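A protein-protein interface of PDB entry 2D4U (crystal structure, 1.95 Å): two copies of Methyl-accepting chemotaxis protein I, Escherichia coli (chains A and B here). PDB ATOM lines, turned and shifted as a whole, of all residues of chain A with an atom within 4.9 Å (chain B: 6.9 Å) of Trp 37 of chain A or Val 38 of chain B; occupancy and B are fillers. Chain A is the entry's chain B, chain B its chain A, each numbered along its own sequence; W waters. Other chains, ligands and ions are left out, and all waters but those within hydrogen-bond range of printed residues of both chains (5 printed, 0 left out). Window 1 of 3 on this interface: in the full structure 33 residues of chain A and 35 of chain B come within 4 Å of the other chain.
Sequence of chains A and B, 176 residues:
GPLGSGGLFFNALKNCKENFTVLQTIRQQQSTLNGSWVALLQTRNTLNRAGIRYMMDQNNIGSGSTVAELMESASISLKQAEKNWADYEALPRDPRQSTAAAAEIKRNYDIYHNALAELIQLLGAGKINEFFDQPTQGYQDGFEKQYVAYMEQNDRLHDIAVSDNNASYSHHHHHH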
ATOM      1  N   LEU A  33      -3.975  -7.265  -5.981  1.00  0.00           N
ATOM      2  CA  LEU A  33      -5.197  -6.502  -6.152  1.00  0.00           C
ATOM      3  C   LEU A  33      -6.241  -7.335  -6.945  1.00  0.00           C
ATOM      4  O   LEU A  33      -7.410  -7.349  -6.592  1.00  0.00           O
ATOM      5  CB  LEU A  33      -4.898  -5.172  -6.855  1.00  0.00           C
ATOM      6  CG  LEU A  33      -6.089  -4.198  -6.951  1.00  0.00           C
ATOM      7  CD1 LEU A  33      -6.708  -3.973  -5.600  1.00  0.00           C
ATOM      8  CD2 LEU A  33      -5.597  -2.908  -7.510  1.00  0.00           C
ATOM      9  N   ASN A  34      -5.818  -8.002  -8.019  1.00  0.00           N
ATOM     10  CA  ASN A  34      -6.742  -8.874  -8.750  1.00  0.00           C
ATOM     11  C   ASN A  34      -7.213 -10.032  -7.865  1.00  0.00           C
ATOM     12  O   ASN A  34      -8.362 -10.404  -7.916  1.00  0.00           O
ATOM     13  CB  ASN A  34      -6.135  -9.427 -10.064  1.00  0.00           C
ATOM     14  CG  ASN A  34      -7.213 -10.034 -11.019  1.00  0.00           C
ATOM     15  OD1 ASN A  34      -7.413 -11.265 -11.083  1.00  0.00           O
ATOM     16  ND2 ASN A  34      -7.877  -9.170 -11.775  1.00  0.00           N
ATOM     17  N   GLY A  35      -6.333 -10.565  -7.007  1.00  0.00           N
ATOM     18  CA  GLY A  35      -6.768 -11.589  -6.088  1.00  0.00           C
ATOM     19  C   GLY A  35      -7.867 -11.110  -5.139  1.00  0.00           C
ATOM     20  O   GLY A  35      -8.834 -11.849  -4.833  1.00  0.00           O
ATOM     21  N   SER A  36      -7.721  -9.879  -4.655  1.00  0.00           N
ATOM     22  CA  SER A  36      -8.704  -9.299  -3.749  1.00  0.00           C
ATOM     23  C   SER A  36     -10.039  -9.128  -4.507  1.00  0.00           C
ATOM     24  O   SER A  36     -11.063  -9.551  -4.032  1.00  0.00           O
ATOM     25  CB  SER A  36      -8.222  -7.974  -3.232  1.00  0.00           C
ATOM     26  OG  SER A  36      -9.096  -7.530  -2.234  1.00  0.00           O
ATOM     27  N   TRP A  37      -9.970  -8.571  -5.704  1.00  0.00           N
ATOM     28  CA  TRP A  37     -11.147  -8.399  -6.591  1.00  0.00           C
ATOM     29  C   TRP A  37     -11.870  -9.717  -6.908  1.00  0.00           C
ATOM     30  O   TRP A  37     -13.103  -9.804  -6.838  1.00  0.00           O
ATOM     31  CB  TRP A  37     -10.630  -7.767  -7.848  1.00  0.00           C
ATOM     32  CG  TRP A  37     -11.561  -7.438  -9.019  1.00  0.00           C
ATOM     33  CD1 TRP A  37     -11.199  -7.485 -10.348  1.00  0.00           C
ATOM     34  CD2 TRP A  37     -12.908  -6.911  -9.003  1.00  0.00           C
ATOM     35  NE1 TRP A  37     -12.225  -7.037 -11.141  1.00  0.00           N
ATOM     36  CE2 TRP A  37     -13.291  -6.696 -10.358  1.00  0.00           C
ATOM     37  CE3 TRP A  37     -13.828  -6.619  -8.003  1.00  0.00           C
ATOM     38  CZ2 TRP A  37     -14.551  -6.213 -10.732  1.00  0.00           C
ATOM     39  CZ3 TRP A  37     -15.105  -6.110  -8.378  1.00  0.00           C
ATOM     40  CH2 TRP A  37     -15.440  -5.925  -9.741  1.00  0.00           C
ATOM     41  N   VAL A  38     -11.113 -10.764  -7.213  1.00  0.00           N
ATOM     42  CA  VAL A  38     -11.714 -12.063  -7.473  1.00  0.00           C
ATOM     43  C   VAL A  38     -12.409 -12.573  -6.231  1.00  0.00           C
ATOM     44  O   VAL A  38     -13.529 -13.082  -6.301  1.00  0.00           O
ATOM     45  CB  VAL A  38     -10.667 -13.107  -7.966  1.00  0.00           C
ATOM     46  CG1 VAL A  38     -11.212 -14.591  -7.779  1.00  0.00           C
ATOM     47  CG2 VAL A  38     -10.243 -12.805  -9.434  1.00  0.00           C
ATOM     48  N   ALA A  39     -11.770 -12.425  -5.059  1.00  0.00           N
ATOM     49  CA  ALA A  39     -12.392 -12.923  -3.866  1.00  0.00           C
ATOM     50  C   ALA A  39     -13.672 -12.149  -3.526  1.00  0.00           C
ATOM     51  O   ALA A  39     -14.616 -12.737  -2.992  1.00  0.00           O
ATOM     52  CB  ALA A  39     -11.395 -12.927  -2.626  1.00  0.00           C
ATOM     53  N   LEU A  40     -13.683 -10.842  -3.768  1.00  0.00           N
ATOM     54  CA  LEU A  40     -14.895 -10.060  -3.547  1.00  0.00           C
ATOM     55  C   LEU A  40     -16.000 -10.551  -4.491  1.00  0.00           C
ATOM     56  O   LEU A  40     -17.130 -10.723  -4.058  1.00  0.00           O
ATOM     57  CB  LEU A  40     -14.687  -8.564  -3.781  1.00  0.00           C
ATOM     58  CG  LEU A  40     -13.800  -7.810  -2.765  1.00  0.00           C
ATOM     59  CD1 LEU A  40     -13.481  -6.357  -3.216  1.00  0.00           C
ATOM     60  CD2 LEU A  40     -14.422  -7.815  -1.380  1.00  0.00           C
ATOM     61  N   LEU A  41     -15.689 -10.692  -5.770  1.00  0.00           N
ATOM     62  CA  LEU A  41     -16.673 -11.220  -6.747  1.00  0.00           C
ATOM     63  C   LEU A  41     -17.262 -12.566  -6.356  1.00  0.00           C
ATOM     64  O   LEU A  41     -18.473 -12.849  -6.531  1.00  0.00           O
ATOM     65  CB  LEU A  41     -16.027 -11.322  -8.126  1.00  0.00           C
ATOM     66  CG  LEU A  41     -15.681  -9.983  -8.793  1.00  0.00           C
ATOM     67  CD1 LEU A  41     -14.789 -10.162 -10.061  1.00  0.00           C
ATOM     68  CD2 LEU A  41     -16.974  -9.198  -9.099  1.00  0.00           C
ATOM     69  N   TYR A 112     -17.309  -1.321  -1.327  1.00  0.00           N
ATOM     70  CA  TYR A 112     -17.694  -2.633  -1.833  1.00  0.00           C
ATOM     71  C   TYR A 112     -17.469  -3.710  -0.767  1.00  0.00           C
ATOM     72  O   TYR A 112     -18.351  -4.505  -0.526  1.00  0.00           O
ATOM     73  CB  TYR A 112     -16.909  -2.938  -3.115  1.00  0.00           C
ATOM     74  CG  TYR A 112     -17.391  -4.175  -3.853  1.00  0.00           C
ATOM     75  CD1 TYR A 112     -18.737  -4.560  -3.818  1.00  0.00           C
ATOM     76  CD2 TYR A 112     -16.497  -4.965  -4.575  1.00  0.00           C
ATOM     77  CE1 TYR A 112     -19.164  -5.713  -4.492  1.00  0.00           C
ATOM     78  CE2 TYR A 112     -16.928  -6.098  -5.251  1.00  0.00           C
ATOM     79  CZ  TYR A 112     -18.243  -6.467  -5.209  1.00  0.00           C
ATOM     80  OH  TYR A 112     -18.652  -7.594  -5.900  1.00  0.00           O
ATOM     81  N   GLN A 140     -20.103  -2.379  -6.372  1.00  0.00           N
ATOM     82  CA  GLN A 140     -19.126  -3.102  -7.169  1.00  0.00           C
ATOM     83  C   GLN A 140     -18.636  -2.252  -8.336  1.00  0.00           C
ATOM     84  O   GLN A 140     -17.430  -2.177  -8.640  1.00  0.00           O
ATOM     85  CB  GLN A 140     -19.717  -4.435  -7.654  1.00  0.00           C
ATOM     86  CG  GLN A 140     -18.764  -5.282  -8.505  1.00  0.00           C
ATOM     87  CD  GLN A 140     -19.384  -6.590  -8.989  1.00  0.00           C
ATOM     88  OE1 GLN A 140     -19.737  -7.434  -8.196  1.00  0.00           O
ATOM     89  NE2 GLN A 140     -19.484  -6.752 -10.297  1.00  0.00           N
ATOM     90  N   PHE A 143     -15.904   0.215  -7.551  1.00  0.00           N
ATOM     91  CA  PHE A 143     -14.583  -0.362  -7.409  1.00  0.00           C
ATOM     92  C   PHE A 143     -14.058  -0.698  -8.784  1.00  0.00           C
ATOM     93  O   PHE A 143     -12.931  -0.406  -9.139  1.00  0.00           O
ATOM     94  CB  PHE A 143     -14.628  -1.640  -6.560  1.00  0.00           C
ATOM     95  CG  PHE A 143     -13.287  -2.316  -6.472  1.00  0.00           C
ATOM     96  CD1 PHE A 143     -12.969  -3.350  -7.307  1.00  0.00           C
ATOM     97  CD2 PHE A 143     -12.314  -1.831  -5.610  1.00  0.00           C
ATOM     98  CE1 PHE A 143     -11.712  -3.958  -7.238  1.00  0.00           C
ATOM     99  CE2 PHE A 143     -11.068  -2.429  -5.548  1.00  0.00           C
ATOM    100  CZ  PHE A 143     -10.775  -3.481  -6.369  1.00  0.00           C
ATOM    101  N   GLU A 144     -14.908  -1.327  -9.579  1.00  0.00           N
ATOM    102  CA  GLU A 144     -14.484  -1.787 -10.873  1.00  0.00           C
ATOM    103  C   GLU A 144     -13.912  -0.659 -11.728  1.00  0.00           C
ATOM    104  O   GLU A 144     -12.869  -0.809 -12.362  1.00  0.00           O
ATOM    105  CB  GLU A 144     -15.666  -2.466 -11.582  1.00  0.00           C
ATOM    106  CG  GLU A 144     -15.295  -3.005 -12.932  1.00  0.00           C
ATOM    107  CD  GLU A 144     -16.522  -3.473 -13.705  1.00  0.00           C
ATOM    108  OE1 GLU A 144     -17.297  -2.616 -14.194  1.00  0.00           O
ATOM    109  OE2 GLU A 144     -16.712  -4.682 -13.810  1.00  0.00           O
ATOM    110  N   TYR A 147     -10.550   0.163 -10.586  1.00  0.00           N
ATOM    111  CA  TYR A 147      -9.696  -0.943 -10.960  1.00  0.00           C
ATOM    112  C   TYR A 147      -9.301  -0.862 -12.454  1.00  0.00           C
ATOM    113  O   TYR A 147      -8.146  -1.058 -12.816  1.00  0.00           O
ATOM    114  CB  TYR A 147     -10.406  -2.245 -10.592  1.00  0.00           C
ATOM    115  CG  TYR A 147      -9.632  -3.484 -10.900  1.00  0.00           C
ATOM    116  CD1 TYR A 147      -8.654  -3.941 -10.035  1.00  0.00           C
ATOM    117  CD2 TYR A 147      -9.891  -4.217 -12.053  1.00  0.00           C
ATOM    118  CE1 TYR A 147      -7.936  -5.088 -10.316  1.00  0.00           C
ATOM    119  CE2 TYR A 147      -9.169  -5.347 -12.349  1.00  0.00           C
ATOM    120  CZ  TYR A 147      -8.204  -5.788 -11.471  1.00  0.00           C
ATOM    121  OH  TYR A 147      -7.476  -6.930 -11.756  1.00  0.00           O
ATOM    122  N   LEU B  33      -5.232 -13.466 -18.572  1.00  0.00           N
ATOM    123  CA  LEU B  33      -5.917 -14.547 -17.874  1.00  0.00           C
ATOM    124  C   LEU B  33      -6.801 -13.998 -16.773  1.00  0.00           C
ATOM    125  O   LEU B  33      -7.899 -14.478 -16.603  1.00  0.00           O
ATOM    126  CB  LEU B  33      -4.916 -15.570 -17.302  1.00  0.00           C
ATOM    127  CG  LEU B  33      -5.441 -16.999 -17.099  1.00  0.00           C
ATOM    128  CD1 LEU B  33      -6.139 -17.583 -18.340  1.00  0.00           C
ATOM    129  CD2 LEU B  33      -4.318 -17.931 -16.583  1.00  0.00           C
ATOM    130  N   ASN B  34      -6.293 -13.026 -16.002  1.00  0.00           N
ATOM    131  CA  ASN B  34      -7.050 -12.402 -14.915  1.00  0.00           C
ATOM    132  C   ASN B  34      -8.335 -11.757 -15.451  1.00  0.00           C
ATOM    133  O   ASN B  34      -9.392 -11.881 -14.846  1.00  0.00           O
ATOM    134  CB  ASN B  34      -6.260 -11.289 -14.252  1.00  0.00           C
ATOM    135  CG  ASN B  34      -5.191 -11.800 -13.288  1.00  0.00           C
ATOM    136  OD1 ASN B  34      -4.443 -11.004 -12.725  1.00  0.00           O
ATOM    137  ND2 ASN B  34      -5.102 -13.113 -13.122  1.00  0.00           N
ATOM    138  N   GLY B  35      -8.208 -11.076 -16.587  1.00  0.00           N
ATOM    139  CA  GLY B  35      -9.336 -10.368 -17.195  1.00  0.00           C
ATOM    140  C   GLY B  35     -10.379 -11.383 -17.649  1.00  0.00           C
ATOM    141  O   GLY B  35     -11.580 -11.171 -17.496  1.00  0.00           O
ATOM    142  N   SER B  36      -9.926 -12.501 -18.189  1.00  0.00           N
ATOM    143  CA  SER B  36     -10.867 -13.575 -18.565  1.00  0.00           C
ATOM    144  C   SER B  36     -11.573 -14.205 -17.342  1.00  0.00           C
ATOM    145  O   SER B  36     -12.795 -14.369 -17.343  1.00  0.00           O
ATOM    146  CB  SER B  36     -10.172 -14.657 -19.371  1.00  0.00           C
ATOM    147  OG  SER B  36     -11.164 -15.489 -19.924  1.00  0.00           O
ATOM    148  N   TRP B  37     -10.807 -14.496 -16.291  1.00  0.00           N
ATOM    149  CA  TRP B  37     -11.336 -15.069 -15.047  1.00  0.00           C
ATOM    150  C   TRP B  37     -12.392 -14.138 -14.411  1.00  0.00           C
ATOM    151  O   TRP B  37     -13.504 -14.563 -14.084  1.00  0.00           O
ATOM    152  CB  TRP B  37     -10.115 -15.316 -14.130  1.00  0.00           C
ATOM    153  CG  TRP B  37     -10.274 -15.839 -12.717  1.00  0.00           C
ATOM    154  CD1 TRP B  37      -9.445 -15.537 -11.661  1.00  0.00           C
ATOM    155  CD2 TRP B  37     -11.193 -16.821 -12.222  1.00  0.00           C
ATOM    156  NE1 TRP B  37      -9.846 -16.214 -10.540  1.00  0.00           N
ATOM    157  CE2 TRP B  37     -10.897 -17.025 -10.852  1.00  0.00           C
ATOM    158  CE3 TRP B  37     -12.258 -17.521 -12.772  1.00  0.00           C
ATOM    159  CZ2 TRP B  37     -11.623 -17.895 -10.040  1.00  0.00           C
ATOM    160  CZ3 TRP B  37     -12.980 -18.389 -11.962  1.00  0.00           C
ATOM    161  CH2 TRP B  37     -12.654 -18.564 -10.608  1.00  0.00           C
ATOM    162  N   VAL B  38     -12.077 -12.863 -14.311  1.00  0.00           N
ATOM    163  CA  VAL B  38     -12.982 -11.880 -13.701  1.00  0.00           C
ATOM    164  C   VAL B  38     -14.283 -11.790 -14.527  1.00  0.00           C
ATOM    165  O   VAL B  38     -15.384 -11.734 -13.977  1.00  0.00           O
ATOM    166  CB  VAL B  38     -12.302 -10.485 -13.663  1.00  0.00           C
ATOM    167  CG1 VAL B  38     -13.299  -9.319 -13.402  1.00  0.00           C
ATOM    168  CG2 VAL B  38     -11.167 -10.466 -12.580  1.00  0.00           C
ATOM    169  N   ALA B  39     -14.142 -11.711 -15.835  1.00  0.00           N
ATOM    170  CA  ALA B  39     -15.332 -11.624 -16.713  1.00  0.00           C
ATOM    171  C   ALA B  39     -16.202 -12.904 -16.607  1.00  0.00           C
ATOM    172  O   ALA B  39     -17.439 -12.820 -16.640  1.00  0.00           O
ATOM    173  CB  ALA B  39     -14.913 -11.334 -18.186  1.00  0.00           C
ATOM    174  N   LEU B  40     -15.584 -14.093 -16.478  1.00  0.00           N
ATOM    175  CA  LEU B  40     -16.382 -15.318 -16.212  1.00  0.00           C
ATOM    176  C   LEU B  40     -17.095 -15.237 -14.872  1.00  0.00           C
ATOM    177  O   LEU B  40     -18.291 -15.587 -14.765  1.00  0.00           O
ATOM    178  CB  LEU B  40     -15.517 -16.592 -16.236  1.00  0.00           C
ATOM    179  CG  LEU B  40     -14.803 -16.896 -17.533  1.00  0.00           C
ATOM    180  CD1 LEU B  40     -13.612 -17.904 -17.297  1.00  0.00           C
ATOM    181  CD2 LEU B  40     -15.824 -17.444 -18.563  1.00  0.00           C
ATOM    182  N   LEU B  41     -16.386 -14.801 -13.817  1.00  0.00           N
ATOM    183  CA  LEU B  41     -17.072 -14.650 -12.547  1.00  0.00           C
ATOM    184  C   LEU B  41     -18.242 -13.632 -12.634  1.00  0.00           C
ATOM    185  O   LEU B  41     -19.256 -13.782 -11.960  1.00  0.00           O
ATOM    186  CB  LEU B  41     -16.085 -14.178 -11.465  1.00  0.00           C
ATOM    187  CG  LEU B  41     -15.043 -15.250 -11.075  1.00  0.00           C
ATOM    188  CD1 LEU B  41     -13.878 -14.596 -10.330  1.00  0.00           C
ATOM    189  CD2 LEU B  41     -15.733 -16.351 -10.217  1.00  0.00           C
ATOM    190  N   GLN B  42     -18.043 -12.561 -13.384  1.00  0.00           N
ATOM    191  CA  GLN B  42     -19.067 -11.540 -13.501  1.00  0.00           C
ATOM    192  C   GLN B  42     -20.304 -12.089 -14.172  1.00  0.00           C
ATOM    193  O   GLN B  42     -21.455 -11.793 -13.752  1.00  0.00           O
ATOM    194  CB  GLN B  42     -18.526 -10.373 -14.287  1.00  0.00           C
ATOM    195  CG  GLN B  42     -17.334  -9.701 -13.596  1.00  0.00           C
ATOM    196  CD  GLN B  42     -17.735  -8.460 -12.911  1.00  0.00           C
ATOM    197  OE1 GLN B  42     -18.402  -8.511 -11.874  1.00  0.00           O
ATOM    198  NE2 GLN B  42     -17.358  -7.316 -13.478  1.00  0.00           N
ATOM    199  N   THR B  43     -20.044 -12.848 -15.228  1.00  0.00           N
ATOM    200  CA  THR B  43     -21.053 -13.514 -16.022  1.00  0.00           C
ATOM    201  C   THR B  43     -21.826 -14.441 -15.114  1.00  0.00           C
ATOM    202  O   THR B  43     -23.052 -14.371 -15.054  1.00  0.00           O
ATOM    203  CB  THR B  43     -20.420 -14.323 -17.178  1.00  0.00           C
ATOM    204  OG1 THR B  43     -19.710 -13.438 -18.040  1.00  0.00           O
ATOM    205  CG2 THR B  43     -21.543 -14.951 -18.065  1.00  0.00           C
ATOM    206  N   ARG B  44     -21.106 -15.263 -14.343  1.00  0.00           N
ATOM    207  CA  ARG B  44     -21.787 -16.159 -13.438  1.00  0.00           C
ATOM    208  C   ARG B  44     -22.677 -15.474 -12.398  1.00  0.00           C
ATOM    209  O   ARG B  44     -23.819 -15.941 -12.127  1.00  0.00           O
ATOM    210  CB  ARG B  44     -20.797 -17.056 -12.675  1.00  0.00           C
ATOM    211  CG  ARG B  44     -21.541 -18.000 -11.730  1.00  0.00           C
ATOM    212  CD  ARG B  44     -20.625 -18.979 -11.006  1.00  0.00           C
ATOM    213  NE  ARG B  44     -21.350 -19.911 -10.148  1.00  0.00           N
ATOM    214  CZ  ARG B  44     -20.805 -20.521  -9.109  1.00  0.00           C
ATOM    215  NH1 ARG B  44     -19.540 -20.283  -8.803  1.00  0.00           N
ATOM    216  NH2 ARG B  44     -21.520 -21.367  -8.361  1.00  0.00           N
ATOM    217  N   SER B  77     -20.570  -9.602 -20.743  1.00  0.00           N
ATOM    218  CA  SER B  77     -19.420  -9.990 -19.929  1.00  0.00           C
ATOM    219  C   SER B  77     -18.816 -11.303 -20.445  1.00  0.00           C
ATOM    220  O   SER B  77     -17.593 -11.486 -20.371  1.00  0.00           O
ATOM    221  CB  SER B  77     -19.826 -10.012 -18.450  1.00  0.00           C
ATOM    222  OG  SER B  77     -20.852 -10.951 -18.296  1.00  0.00           O
ATOM    223  N   ALA B  81     -14.946 -12.110 -21.437  1.00  0.00           N
ATOM    224  CA  ALA B  81     -14.158 -13.305 -21.070  1.00  0.00           C
ATOM    225  C   ALA B  81     -13.503 -13.861 -22.305  1.00  0.00           C
ATOM    226  O   ALA B  81     -12.317 -14.203 -22.292  1.00  0.00           O
ATOM    227  CB  ALA B  81     -15.065 -14.421 -20.438  1.00  0.00           C
ATOM    228  N   PHE B 143     -11.597 -24.757 -13.124  1.00  0.00           N
ATOM    229  CA  PHE B 143     -10.811 -23.732 -13.772  1.00  0.00           C
ATOM    230  C   PHE B 143      -9.943 -23.007 -12.749  1.00  0.00           C
ATOM    231  O   PHE B 143      -8.769 -22.726 -12.977  1.00  0.00           O
ATOM    232  CB  PHE B 143     -11.728 -22.726 -14.472  1.00  0.00           C
ATOM    233  CG  PHE B 143     -10.991 -21.554 -14.992  1.00  0.00           C
ATOM    234  CD1 PHE B 143     -10.332 -21.641 -16.197  1.00  0.00           C
ATOM    235  CD2 PHE B 143     -10.846 -20.408 -14.226  1.00  0.00           C
ATOM    236  CE1 PHE B 143      -9.577 -20.602 -16.672  1.00  0.00           C
ATOM    237  CE2 PHE B 143     -10.119 -19.349 -14.713  1.00  0.00           C
ATOM    238  CZ  PHE B 143      -9.465 -19.459 -15.941  1.00  0.00           C
ATOM    239  N   TYR B 147      -5.950 -22.255 -12.629  1.00  0.00           N
ATOM    240  CA  TYR B 147      -5.571 -20.846 -12.609  1.00  0.00           C
ATOM    241  C   TYR B 147      -4.496 -20.608 -11.546  1.00  0.00           C
ATOM    242  O   TYR B 147      -3.466 -19.994 -11.830  1.00  0.00           O
ATOM    243  CB  TYR B 147      -6.830 -19.990 -12.358  1.00  0.00           C
ATOM    244  CG  TYR B 147      -6.557 -18.516 -12.155  1.00  0.00           C
ATOM    245  CD1 TYR B 147      -6.513 -17.637 -13.237  1.00  0.00           C
ATOM    246  CD2 TYR B 147      -6.354 -17.997 -10.869  1.00  0.00           C
ATOM    247  CE1 TYR B 147      -6.268 -16.283 -13.046  1.00  0.00           C
ATOM    248  CE2 TYR B 147      -6.104 -16.648 -10.670  1.00  0.00           C
ATOM    249  CZ  TYR B 147      -6.058 -15.809 -11.766  1.00  0.00           C
ATOM    250  OH  TYR B 147      -5.824 -14.483 -11.556  1.00  0.00           O
HETATM  251  O   HOH W   1     -20.241  -9.625 -10.124  1.00  0.00           O
HETATM  252  O   HOH W   2     -18.604 -14.571  -9.383  1.00  0.00           O
HETATM  253  O   HOH W   3     -21.286  -7.258 -12.750  1.00  0.00           O
HETATM  254  O   HOH W   4     -18.685  -5.623 -15.840  1.00  0.00           O
HETATM  255  O   HOH W   5      -6.418 -13.411  -9.302  1.00  0.00           O
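OD1 of Asn 34 of chain B lies close to OD1 of Asn 34 of chain A (3.4 Å).
The side-chain carboxylate of Glu 144 of chain A lies within hydrogen-bond range of the side-chain amide nitrogen of Gln 42 of chain B, 2.7 Å away.
The side-chain amide oxygen of Gln 42 of chain B lies within hydrogen-bond range of the side-chain amide nitrogen of Gln 140 of chain A, 2.6 Å away.
OE1 of Gln 140 of chain A lies within hydrogen-bond range of OH of Tyr 112 of chain A (2.5 Å).
Among the printed residues, merely in contact across the chains: Leu 41 of chain A with Gln 42 of chain B (3.2 Å), Trp 37 of chain A with Val 38 of chain B (3.4 Å), Val 38 of chain A with Trp 37 of chain B (3.5 Å), Asn 34 of chain A with Tyr 147 of chain B (3.6 Å), Asn 34 of chain A with Val 38 of chain B (3.6 Å), Val 38 of chain A with Leu 41 of chain B (3.7 Å) and Leu 41 of chain A with Val 38 of chain B (3.8 Å).
Of chain B, only Val 38 (3.4 Å) comes within 4 Å of Trp 37 of chain A.
Of the printed residues of chain A, Asn 34 of chain B touches Asn 34 (3.2 Å).
Printed residues of chain A within 4 Å of Trp 37 of chain B: Val 38.
The nearest residue of chain A that does not touch Val 38 of chain B is Val 38 of chain A (4.03 Å).
Printed residues of chain A that touch a printed residue of chain B: Asn 34, Trp 37, Val 38, Leu 41, Gln 140 and Glu 144.
Hydrophobic or aromatic side chains of chain A that line the printed part of chain B: Trp 37, Val 38 and Leu 41.
Along chain A the printed residues that touch a printed residue of chain B span positions 34 to 144.
Printed residues of chain B that touch a printed residue of chain A: Asn 34, Trp 37, Val 38, Leu 41, Gln 42 and Tyr 147.
Hydrophobic or aromatic side chains of chain B that line the printed part of chain A: Trp 37, Val 38, Leu 41 and Tyr 147.
Among the printed residues, 10 pairs touch across the chains.
Asn 34 of chain B touches its own counterpart, Asn 34 of chain A.
Asn 34 of chain A touches Val 38 of chain B, but with the chains exchanged Val 38 of chain A does not touch Asn 34 of chain B (5.6 Å).
Asn 34 of chain A touches Tyr 147 of chain B, but with the chains exchanged Tyr 147 of chain A does not touch Asn 34 of chain B (5.2 Å).
Val 38 of chain A touches Leu 41 of chain B, and with the chains exchanged Leu 41 of chain A touches Val 38 of chain B.
11 positions are printed for both chains.
Of the 10 pairs that touch across the chains among the printed residues, 5 have their exchanged pair printed and touching as well.
Water W5 bridges the side-chain hydroxyl of Tyr 147 of chain B and the side-chain amide oxygen of Asn 34 of chain A.
Water W1 lies within hydrogen-bond range of the side-chain amide oxygen of Gln 42 of chain B (2.8 Å) and the side-chain amide oxygen of Gln 140 of chain A (3.0 Å).
Water W2 lies within hydrogen-bond range of O of Leu 41 of chain B (2.8 Å) and O of Leu 41 of chain A (3.3 Å).
Water W4 lies within hydrogen-bond range of the side-chain carboxylate of Glu 144 of chain A (3.0 Å) and the side-chain amide nitrogen of Gln 42 of chain B (3.2 Å).
Water W3 lies within hydrogen-bond range of the side-chain amide nitrogen of Gln 140 of chain A (3.1 Å) and the side-chain amide oxygen of Gln 42 of chain B (3.3 Å).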
